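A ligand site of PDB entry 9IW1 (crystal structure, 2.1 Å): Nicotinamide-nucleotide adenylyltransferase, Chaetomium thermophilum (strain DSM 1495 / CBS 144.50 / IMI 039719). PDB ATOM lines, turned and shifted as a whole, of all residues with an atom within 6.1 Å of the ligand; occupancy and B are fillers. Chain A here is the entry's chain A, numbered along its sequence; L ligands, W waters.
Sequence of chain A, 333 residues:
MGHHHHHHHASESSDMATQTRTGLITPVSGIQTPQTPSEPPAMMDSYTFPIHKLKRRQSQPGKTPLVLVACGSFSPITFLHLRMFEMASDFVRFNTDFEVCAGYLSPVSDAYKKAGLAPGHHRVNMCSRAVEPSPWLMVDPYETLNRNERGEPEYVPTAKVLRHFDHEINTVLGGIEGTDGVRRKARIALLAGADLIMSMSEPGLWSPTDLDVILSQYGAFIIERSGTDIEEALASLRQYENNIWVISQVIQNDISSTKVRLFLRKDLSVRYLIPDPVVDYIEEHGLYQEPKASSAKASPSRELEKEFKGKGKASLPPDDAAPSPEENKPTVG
An oxygen (O7) of the ligand lies within hydrogen-bond range of the side-chain hydroxyl of Tyr 155 (2.7 Å).
The side-chain amino group (NZ) of Lys 114 lies within salt-bridge range of an oxygen (O2) of the ligand, 2.7 Å away.
O of Leu 205 lies within hydrogen-bond range of N2 of the ligand, at 2.8 Å.
The backbone NH (N) of Ser 73 sits at hydrogen-bond distance from an oxygen (O1) of the ligand (3.0 Å).
The side-chain hydroxyl (OG) of Ser 73 lies within hydrogen-bond range of an oxygen (O1) of the ligand, 3.3 Å away.
O8 of the ligand lies within hydrogen-bond range of N of Thr 158.
Water W5 lies within hydrogen-bond range of an oxygen (O6) of the ligand (2.5 Å), the side-chain carboxylate (OE2) of Glu 143 (2.8 Å), the backbone carbonyl oxygen (O) of Ser 106 (3.0 Å), the backbone NH (N) of Gly 72 (3.4 Å) and the backbone NH (N) of Val 108 (3.5 Å).
Water W3 lies within hydrogen-bond range of the side-chain carboxylate (OD2) of Asp 210, a nitrogen (N2) of the ligand and the backbone NH (N) of Ser 207.
Water W2 lies within hydrogen-bond range of the side-chain hydroxyl of Tyr 112 (2.4 Å) and an oxygen (O2) of the ligand (2.7 Å).
Water W6 lies within hydrogen-bond range of an oxygen (O1) of the ligand (2.8 Å), the backbone NH of Phe 74 (2.9 Å), the backbone NH of Ser 73 (3.2 Å) and a ring nitrogen (NE2) of His 81 (3.4 Å).
Water W4 lies within hydrogen-bond range of the side-chain carboxylate of Asp 210 (2.6 Å), an oxygen (O8) of the ligand (2.9 Å), the backbone NH of Ala 159 (3.0 Å) and the backbone NH of Thr 158 (3.3 Å).
Water W7 bridges the backbone carbonyl oxygen of Cys 71 (2.9 Å) and an oxygen (O3) of the ligand (3.2 Å).
NE1 of Trp 206 lies within hydrogen-bond range of OG of Ser 199, 2.9 Å away.
The backbone NH (N) of Val 108 sits at hydrogen-bond distance from the backbone carbonyl oxygen (O) of Gly 72 (2.9 Å).
N of Gly 72 sits at hydrogen-bond distance from O of Ser 106, 3.4 Å away.
SG of Cys 71 is in hydrogen-bond range of OE2 of Glu 143, 3.7 Å away.
Cys 71 touches the ligand.
CA of Gly 72 touches O4 of the ligand, 3.3 Å away.
CG2 of Val 108 touches O7 of the ligand, at 3.5 Å.
Tyr 112 touches the ligand.
Pro 157 touches the ligand.
Leu 196 touches the ligand.
Trp 206 touches the ligand.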
ATOM      1  N   CYS A  71      19.824 -23.947  23.959  1.00  0.00           N
ATOM      2  CA  CYS A  71      20.689 -24.496  22.920  1.00  0.00           C
ATOM      3  C   CYS A  71      21.952 -25.075  23.537  1.00  0.00           C
ATOM      4  O   CYS A  71      22.684 -24.372  24.243  1.00  0.00           O
ATOM      5  CB  CYS A  71      21.071 -23.401  21.919  1.00  0.00           C
ATOM      6  SG  CYS A  71      19.757 -22.867  20.820  1.00  0.00           S
ATOM      7  N   GLY A  72      22.208 -26.350  23.256  1.00  0.00           N
ATOM      8  CA  GLY A  72      23.404 -26.977  23.794  1.00  0.00           C
ATOM      9  C   GLY A  72      23.673 -28.291  23.102  1.00  0.00           C
ATOM     10  O   GLY A  72      22.906 -28.735  22.227  1.00  0.00           O
ATOM     11  N   SER A  73      24.767 -28.931  23.513  1.00  0.00           N
ATOM     12  CA  SER A  73      25.115 -30.240  22.967  1.00  0.00           C
ATOM     13  C   SER A  73      24.224 -31.325  23.560  1.00  0.00           C
ATOM     14  O   SER A  73      23.731 -32.200  22.838  1.00  0.00           O
ATOM     15  CB  SER A  73      26.582 -30.561  23.250  1.00  0.00           C
ATOM     16  OG  SER A  73      27.447 -29.585  22.690  1.00  0.00           O
ATOM     17  N   PHE A  74      23.999 -31.278  24.869  1.00  0.00           N
ATOM     18  CA  PHE A  74      23.227 -32.305  25.568  1.00  0.00           C
ATOM     19  C   PHE A  74      23.776 -33.694  25.258  1.00  0.00           C
ATOM     20  O   PHE A  74      23.082 -34.566  24.726  1.00  0.00           O
ATOM     21  CB  PHE A  74      21.745 -32.184  25.230  1.00  0.00           C
ATOM     22  CG  PHE A  74      21.179 -30.809  25.510  1.00  0.00           C
ATOM     23  CD1 PHE A  74      21.170 -30.309  26.805  1.00  0.00           C
ATOM     24  CD2 PHE A  74      20.687 -30.021  24.482  1.00  0.00           C
ATOM     25  CE1 PHE A  74      20.668 -29.044  27.074  1.00  0.00           C
ATOM     26  CE2 PHE A  74      20.161 -28.737  24.744  1.00  0.00           C
ATOM     27  CZ  PHE A  74      20.160 -28.264  26.044  1.00  0.00           C
ATOM     28  N   HIS A  81      21.120 -29.277  33.564  1.00  0.00           N
ATOM     29  CA  HIS A  81      20.431 -28.688  32.412  1.00  0.00           C
ATOM     30  C   HIS A  81      18.947 -28.543  32.706  1.00  0.00           C
ATOM     31  O   HIS A  81      18.344 -27.514  32.393  1.00  0.00           O
ATOM     32  CB  HIS A  81      20.626 -29.554  31.165  1.00  0.00           C
ATOM     33  CG  HIS A  81      22.052 -29.657  30.699  1.00  0.00           C
ATOM     34  ND1 HIS A  81      22.653 -30.872  30.417  1.00  0.00           N
ATOM     35  CD2 HIS A  81      22.967 -28.714  30.416  1.00  0.00           C
ATOM     36  CE1 HIS A  81      23.890 -30.664  30.015  1.00  0.00           C
ATOM     37  NE2 HIS A  81      24.108 -29.364  30.001  1.00  0.00           N
ATOM     38  N   SER A 106      17.126 -27.682  22.621  1.00  0.00           N
ATOM     39  CA  SER A 106      17.506 -27.637  21.213  1.00  0.00           C
ATOM     40  C   SER A 106      18.885 -28.259  21.059  1.00  0.00           C
ATOM     41  O   SER A 106      19.899 -27.555  21.112  1.00  0.00           O
ATOM     42  CB  SER A 106      17.478 -26.191  20.706  1.00  0.00           C
ATOM     43  OG  SER A 106      17.608 -26.152  19.299  1.00  0.00           O
ATOM     44  N   VAL A 108      22.288 -29.531  19.548  1.00  0.00           N
ATOM     45  CA  VAL A 108      23.050 -28.969  18.448  1.00  0.00           C
ATOM     46  C   VAL A 108      23.224 -29.992  17.332  1.00  0.00           C
ATOM     47  O   VAL A 108      23.125 -31.210  17.530  1.00  0.00           O
ATOM     48  CB  VAL A 108      24.411 -28.456  18.961  1.00  0.00           C
ATOM     49  CG1 VAL A 108      25.407 -29.622  19.157  1.00  0.00           C
ATOM     50  CG2 VAL A 108      24.994 -27.385  18.043  1.00  0.00           C
ATOM     51  N   TYR A 112      28.493 -29.683  14.535  1.00  0.00           N
ATOM     52  CA  TYR A 112      29.203 -28.820  15.472  1.00  0.00           C
ATOM     53  C   TYR A 112      30.588 -29.362  15.774  1.00  0.00           C
ATOM     54  O   TYR A 112      30.748 -30.528  16.129  1.00  0.00           O
ATOM     55  CB  TYR A 112      28.397 -28.664  16.761  1.00  0.00           C
ATOM     56  CG  TYR A 112      28.865 -27.564  17.705  1.00  0.00           C
ATOM     57  CD1 TYR A 112      28.998 -26.245  17.268  1.00  0.00           C
ATOM     58  CD2 TYR A 112      29.093 -27.824  19.047  1.00  0.00           C
ATOM     59  CE1 TYR A 112      29.395 -25.236  18.148  1.00  0.00           C
ATOM     60  CE2 TYR A 112      29.487 -26.832  19.916  1.00  0.00           C
ATOM     61  CZ  TYR A 112      29.634 -25.538  19.477  1.00  0.00           C
ATOM     62  OH  TYR A 112      30.036 -24.561  20.369  1.00  0.00           O
ATOM     63  N   LYS A 113      31.599 -28.501  15.643  1.00  0.00           N
ATOM     64  CA  LYS A 113      32.979 -28.861  15.978  1.00  0.00           C
ATOM     65  C   LYS A 113      33.188 -29.018  17.487  1.00  0.00           C
ATOM     66  O   LYS A 113      33.696 -28.102  18.136  1.00  0.00           O
ATOM     67  CB  LYS A 113      33.929 -27.803  15.411  1.00  0.00           C
ATOM     68  CG  LYS A 113      33.422 -26.343  15.512  1.00  0.00           C
ATOM     69  CD  LYS A 113      34.313 -25.505  16.441  1.00  0.00           C
ATOM     70  CE  LYS A 113      33.556 -24.943  17.647  1.00  0.00           C
ATOM     71  NZ  LYS A 113      32.524 -23.955  17.226  1.00  0.00           N
ATOM     72  N   LYS A 114      32.757 -30.147  18.064  1.00  0.00           N
ATOM     73  CA  LYS A 114      32.987 -30.399  19.489  1.00  0.00           C
ATOM     74  C   LYS A 114      33.238 -31.885  19.723  1.00  0.00           C
ATOM     75  O   LYS A 114      32.736 -32.729  18.971  1.00  0.00           O
ATOM     76  CB  LYS A 114      31.795 -29.901  20.314  1.00  0.00           C
ATOM     77  CG  LYS A 114      32.070 -29.715  21.800  1.00  0.00           C
ATOM     78  CD  LYS A 114      30.878 -29.082  22.495  1.00  0.00           C
ATOM     79  CE  LYS A 114      30.562 -29.776  23.812  1.00  0.00           C
ATOM     80  NZ  LYS A 114      30.344 -28.828  24.928  1.00  0.00           N
ATOM     81  N   GLU A 143      17.481 -28.644  14.908  1.00  0.00           N
ATOM     82  CA  GLU A 143      18.888 -28.453  14.585  1.00  0.00           C
ATOM     83  C   GLU A 143      19.538 -29.748  14.089  1.00  0.00           C
ATOM     84  O   GLU A 143      20.382 -29.709  13.192  1.00  0.00           O
ATOM     85  CB  GLU A 143      19.660 -27.908  15.784  1.00  0.00           C
ATOM     86  CG  GLU A 143      19.360 -26.462  16.145  1.00  0.00           C
ATOM     87  CD  GLU A 143      20.344 -25.918  17.186  1.00  0.00           C
ATOM     88  OE1 GLU A 143      21.546 -25.764  16.864  1.00  0.00           O
ATOM     89  OE2 GLU A 143      19.903 -25.668  18.333  1.00  0.00           O
ATOM     90  N   TYR A 155      25.375 -27.217  10.340  1.00  0.00           N
ATOM     91  CA  TYR A 155      25.271 -26.488  11.593  1.00  0.00           C
ATOM     92  C   TYR A 155      24.312 -25.317  11.476  1.00  0.00           C
ATOM     93  O   TYR A 155      24.306 -24.602  10.474  1.00  0.00           O
ATOM     94  CB  TYR A 155      26.663 -26.004  12.008  1.00  0.00           C
ATOM     95  CG  TYR A 155      26.641 -25.133  13.217  1.00  0.00           C
ATOM     96  CD1 TYR A 155      26.419 -25.677  14.473  1.00  0.00           C
ATOM     97  CD2 TYR A 155      26.829 -23.768  13.123  1.00  0.00           C
ATOM     98  CE1 TYR A 155      26.378 -24.889  15.590  1.00  0.00           C
ATOM     99  CE2 TYR A 155      26.809 -22.967  14.233  1.00  0.00           C
ATOM    100  CZ  TYR A 155      26.578 -23.530  15.462  1.00  0.00           C
ATOM    101  OH  TYR A 155      26.561 -22.737  16.584  1.00  0.00           O
ATOM    102  N   VAL A 156      23.502 -25.097  12.521  1.00  0.00           N
ATOM    103  CA  VAL A 156      22.531 -24.007  12.563  1.00  0.00           C
ATOM    104  C   VAL A 156      23.034 -22.992  13.581  1.00  0.00           C
ATOM    105  O   VAL A 156      23.031 -23.273  14.786  1.00  0.00           O
ATOM    106  CB  VAL A 156      21.131 -24.510  12.935  1.00  0.00           C
ATOM    107  CG1 VAL A 156      20.104 -23.416  12.710  1.00  0.00           C
ATOM    108  CG2 VAL A 156      20.773 -25.777  12.163  1.00  0.00           C
ATOM    109  N   PRO A 157      23.445 -21.801  13.162  1.00  0.00           N
ATOM    110  CA  PRO A 157      23.848 -20.790  14.136  1.00  0.00           C
ATOM    111  C   PRO A 157      22.692 -20.386  15.029  1.00  0.00           C
ATOM    112  O   PRO A 157      21.512 -20.465  14.665  1.00  0.00           O
ATOM    113  CB  PRO A 157      24.334 -19.624  13.264  1.00  0.00           C
ATOM    114  CG  PRO A 157      23.768 -19.879  11.915  1.00  0.00           C
ATOM    115  CD  PRO A 157      23.659 -21.362  11.771  1.00  0.00           C
ATOM    116  N   THR A 158      23.042 -19.956  16.243  1.00  0.00           N
ATOM    117  CA  THR A 158      22.044 -19.745  17.277  1.00  0.00           C
ATOM    118  C   THR A 158      21.018 -18.696  16.850  1.00  0.00           C
ATOM    119  O   THR A 158      19.823 -18.863  17.092  1.00  0.00           O
ATOM    120  CB  THR A 158      22.749 -19.340  18.570  1.00  0.00           C
ATOM    121  OG1 THR A 158      23.527 -20.440  19.054  1.00  0.00           O
ATOM    122  CG2 THR A 158      21.742 -18.940  19.625  1.00  0.00           C
ATOM    123  N   ALA A 159      21.468 -17.643  16.158  1.00  0.00           N
ATOM    124  CA  ALA A 159      20.522 -16.654  15.651  1.00  0.00           C
ATOM    125  C   ALA A 159      19.481 -17.301  14.741  1.00  0.00           C
ATOM    126  O   ALA A 159      18.289 -16.974  14.824  1.00  0.00           O
ATOM    127  CB  ALA A 159      21.261 -15.549  14.890  1.00  0.00           C
ATOM    128  N   LEU A 196      28.130 -19.431  28.430  1.00  0.00           N
ATOM    129  CA  LEU A 196      27.646 -18.939  27.148  1.00  0.00           C
ATOM    130  C   LEU A 196      27.848 -17.430  27.004  1.00  0.00           C
ATOM    131  O   LEU A 196      28.229 -16.952  25.935  1.00  0.00           O
ATOM    132  CB  LEU A 196      26.179 -19.311  26.982  1.00  0.00           C
ATOM    133  CG  LEU A 196      25.587 -19.419  25.571  1.00  0.00           C
ATOM    134  CD1 LEU A 196      25.474 -18.092  24.873  1.00  0.00           C
ATOM    135  CD2 LEU A 196      26.437 -20.393  24.755  1.00  0.00           C
ATOM    136  N   SER A 199      31.438 -16.882  26.315  1.00  0.00           N
ATOM    137  CA  SER A 199      31.706 -17.216  24.922  1.00  0.00           C
ATOM    138  C   SER A 199      31.245 -16.098  23.984  1.00  0.00           C
ATOM    139  O   SER A 199      31.956 -15.737  23.038  1.00  0.00           O
ATOM    140  CB  SER A 199      30.998 -18.532  24.568  1.00  0.00           C
ATOM    141  OG  SER A 199      30.998 -18.757  23.167  1.00  0.00           O
ATOM    142  N   LEU A 205      33.881 -16.440  17.805  1.00  0.00           N
ATOM    143  CA  LEU A 205      32.801 -17.409  17.644  1.00  0.00           C
ATOM    144  C   LEU A 205      31.482 -16.783  17.221  1.00  0.00           C
ATOM    145  O   LEU A 205      30.694 -17.448  16.546  1.00  0.00           O
ATOM    146  CB  LEU A 205      32.633 -18.251  18.909  1.00  0.00           C
ATOM    147  CG  LEU A 205      33.954 -18.865  19.392  1.00  0.00           C
ATOM    148  CD1 LEU A 205      33.763 -19.682  20.680  1.00  0.00           C
ATOM    149  CD2 LEU A 205      34.594 -19.702  18.285  1.00  0.00           C
ATOM    150  N   TRP A 206      31.219 -15.531  17.601  1.00  0.00           N
ATOM    151  CA  TRP A 206      29.942 -14.879  17.321  1.00  0.00           C
ATOM    152  C   TRP A 206      30.133 -13.659  16.422  1.00  0.00           C
ATOM    153  O   TRP A 206      30.810 -12.702  16.815  1.00  0.00           O
ATOM    154  CB  TRP A 206      29.275 -14.465  18.631  1.00  0.00           C
ATOM    155  CG  TRP A 206      29.150 -15.589  19.607  1.00  0.00           C
ATOM    156  CD1 TRP A 206      30.126 -16.076  20.428  1.00  0.00           C
ATOM    157  CD2 TRP A 206      27.974 -16.354  19.882  1.00  0.00           C
ATOM    158  NE1 TRP A 206      29.643 -17.114  21.183  1.00  0.00           N
ATOM    159  CE2 TRP A 206      28.323 -17.304  20.866  1.00  0.00           C
ATOM    160  CE3 TRP A 206      26.671 -16.350  19.374  1.00  0.00           C
ATOM    161  CZ2 TRP A 206      27.399 -18.226  21.374  1.00  0.00           C
ATOM    162  CZ3 TRP A 206      25.761 -17.273  19.877  1.00  0.00           C
ATOM    163  CH2 TRP A 206      26.134 -18.184  20.870  1.00  0.00           C
ATOM    164  N   SER A 207      29.479 -13.680  15.257  1.00  0.00           N
ATOM    165  CA  SER A 207      29.490 -12.508  14.372  1.00  0.00           C
ATOM    166  C   SER A 207      28.710 -11.351  14.999  1.00  0.00           C
ATOM    167  O   SER A 207      27.730 -11.572  15.706  1.00  0.00           O
ATOM    168  CB  SER A 207      28.891 -12.854  13.008  1.00  0.00           C
ATOM    169  OG  SER A 207      27.493 -12.647  13.014  1.00  0.00           O
ATOM    170  N   ASP A 210      24.873 -11.476  14.256  1.00  0.00           N
ATOM    171  CA  ASP A 210      24.133 -12.474  15.016  1.00  0.00           C
ATOM    172  C   ASP A 210      23.964 -12.041  16.471  1.00  0.00           C
ATOM    173  O   ASP A 210      22.867 -12.142  17.029  1.00  0.00           O
ATOM    174  CB  ASP A 210      24.846 -13.818  14.939  1.00  0.00           C
ATOM    175  CG  ASP A 210      24.625 -14.505  13.608  1.00  0.00           C
ATOM    176  OD1 ASP A 210      24.051 -13.859  12.703  1.00  0.00           O
ATOM    177  OD2 ASP A 210      25.048 -15.674  13.477  1.00  0.00           O
ATOM    178  N   ILE A 214      20.489 -11.845  18.228  1.00  0.00           N
ATOM    179  CA  ILE A 214      20.232 -12.678  19.386  1.00  0.00           C
ATOM    180  C   ILE A 214      19.851 -11.843  20.599  1.00  0.00           C
ATOM    181  O   ILE A 214      18.876 -12.117  21.296  1.00  0.00           O
ATOM    182  CB  ILE A 214      21.461 -13.564  19.678  1.00  0.00           C
ATOM    183  CG1 ILE A 214      21.629 -14.626  18.590  1.00  0.00           C
ATOM    184  CG2 ILE A 214      21.356 -14.201  21.056  1.00  0.00           C
ATOM    185  CD1 ILE A 214      22.850 -15.508  18.799  1.00  0.00           C
HETATM  186  O1  LIG L   1      26.782 -27.655  25.305  1.00  0.00           O
HETATM  187  P1  LIG L   1      27.445 -26.363  24.843  1.00  0.00           P
HETATM  188  O2  LIG L   1      28.771 -26.712  24.205  1.00  0.00           O
HETATM  189  O3  LIG L   1      27.666 -25.474  26.052  1.00  0.00           O
HETATM  190  O4  LIG L   1      26.439 -25.580  23.771  1.00  0.00           O
HETATM  191  C1  LIG L   1      26.883 -24.479  22.981  1.00  0.00           C
HETATM  192  C2  LIG L   1      25.705 -23.900  22.201  1.00  0.00           C
HETATM  193  O5  LIG L   1      26.055 -22.386  21.730  1.00  0.00           O
HETATM  194  C3  LIG L   1      25.467 -24.590  21.116  1.00  0.00           C
HETATM  195  O6  LIG L   1      24.007 -24.579  20.778  1.00  0.00           O
HETATM  196  C4  LIG L   1      26.216 -23.829  20.001  1.00  0.00           C
HETATM  197  O7  LIG L   1      25.622 -24.031  18.788  1.00  0.00           O
HETATM  198  C5  LIG L   1      25.985 -22.382  20.420  1.00  0.00           C
HETATM  199  N1  LIG L   1      27.032 -21.533  19.803  1.00  0.00           N
HETATM  200  C6  LIG L   1      26.644 -20.711  18.808  1.00  0.00           C
HETATM  201  C7  LIG L   1      27.572 -19.898  18.186  1.00  0.00           C
HETATM  202  C8  LIG L   1      27.054 -18.984  17.072  1.00  0.00           C
HETATM  203  O8  LIG L   1      25.911 -19.063  16.758  1.00  0.00           O
HETATM  204  N2  LIG L   1      27.947 -18.025  16.433  1.00  0.00           N
HETATM  205  C9  LIG L   1      28.879 -19.926  18.556  1.00  0.00           C
HETATM  206  C10 LIG L   1      29.269 -20.763  19.557  1.00  0.00           C
HETATM  207  C11 LIG L   1      28.329 -21.593  20.190  1.00  0.00           C
HETATM  208  O   HOH W   1      22.826 -23.652  17.477  1.00  0.00           O
HETATM  209  O   HOH W   2      29.886 -24.706  22.771  1.00  0.00           O
HETATM  210  O   HOH W   3      27.400 -16.209  14.523  1.00  0.00           O
HETATM  211  O   HOH W   4      24.301 -17.038  15.527  1.00  0.00           O
HETATM  212  O   HOH W   5      22.247 -26.071  19.891  1.00  0.00           O
HETATM  213  O   HOH W   6      24.996 -29.333  26.713  1.00  0.00           O
HETATM  214  O   HOH W   7      24.810 -23.945  26.226  1.00  0.00           O
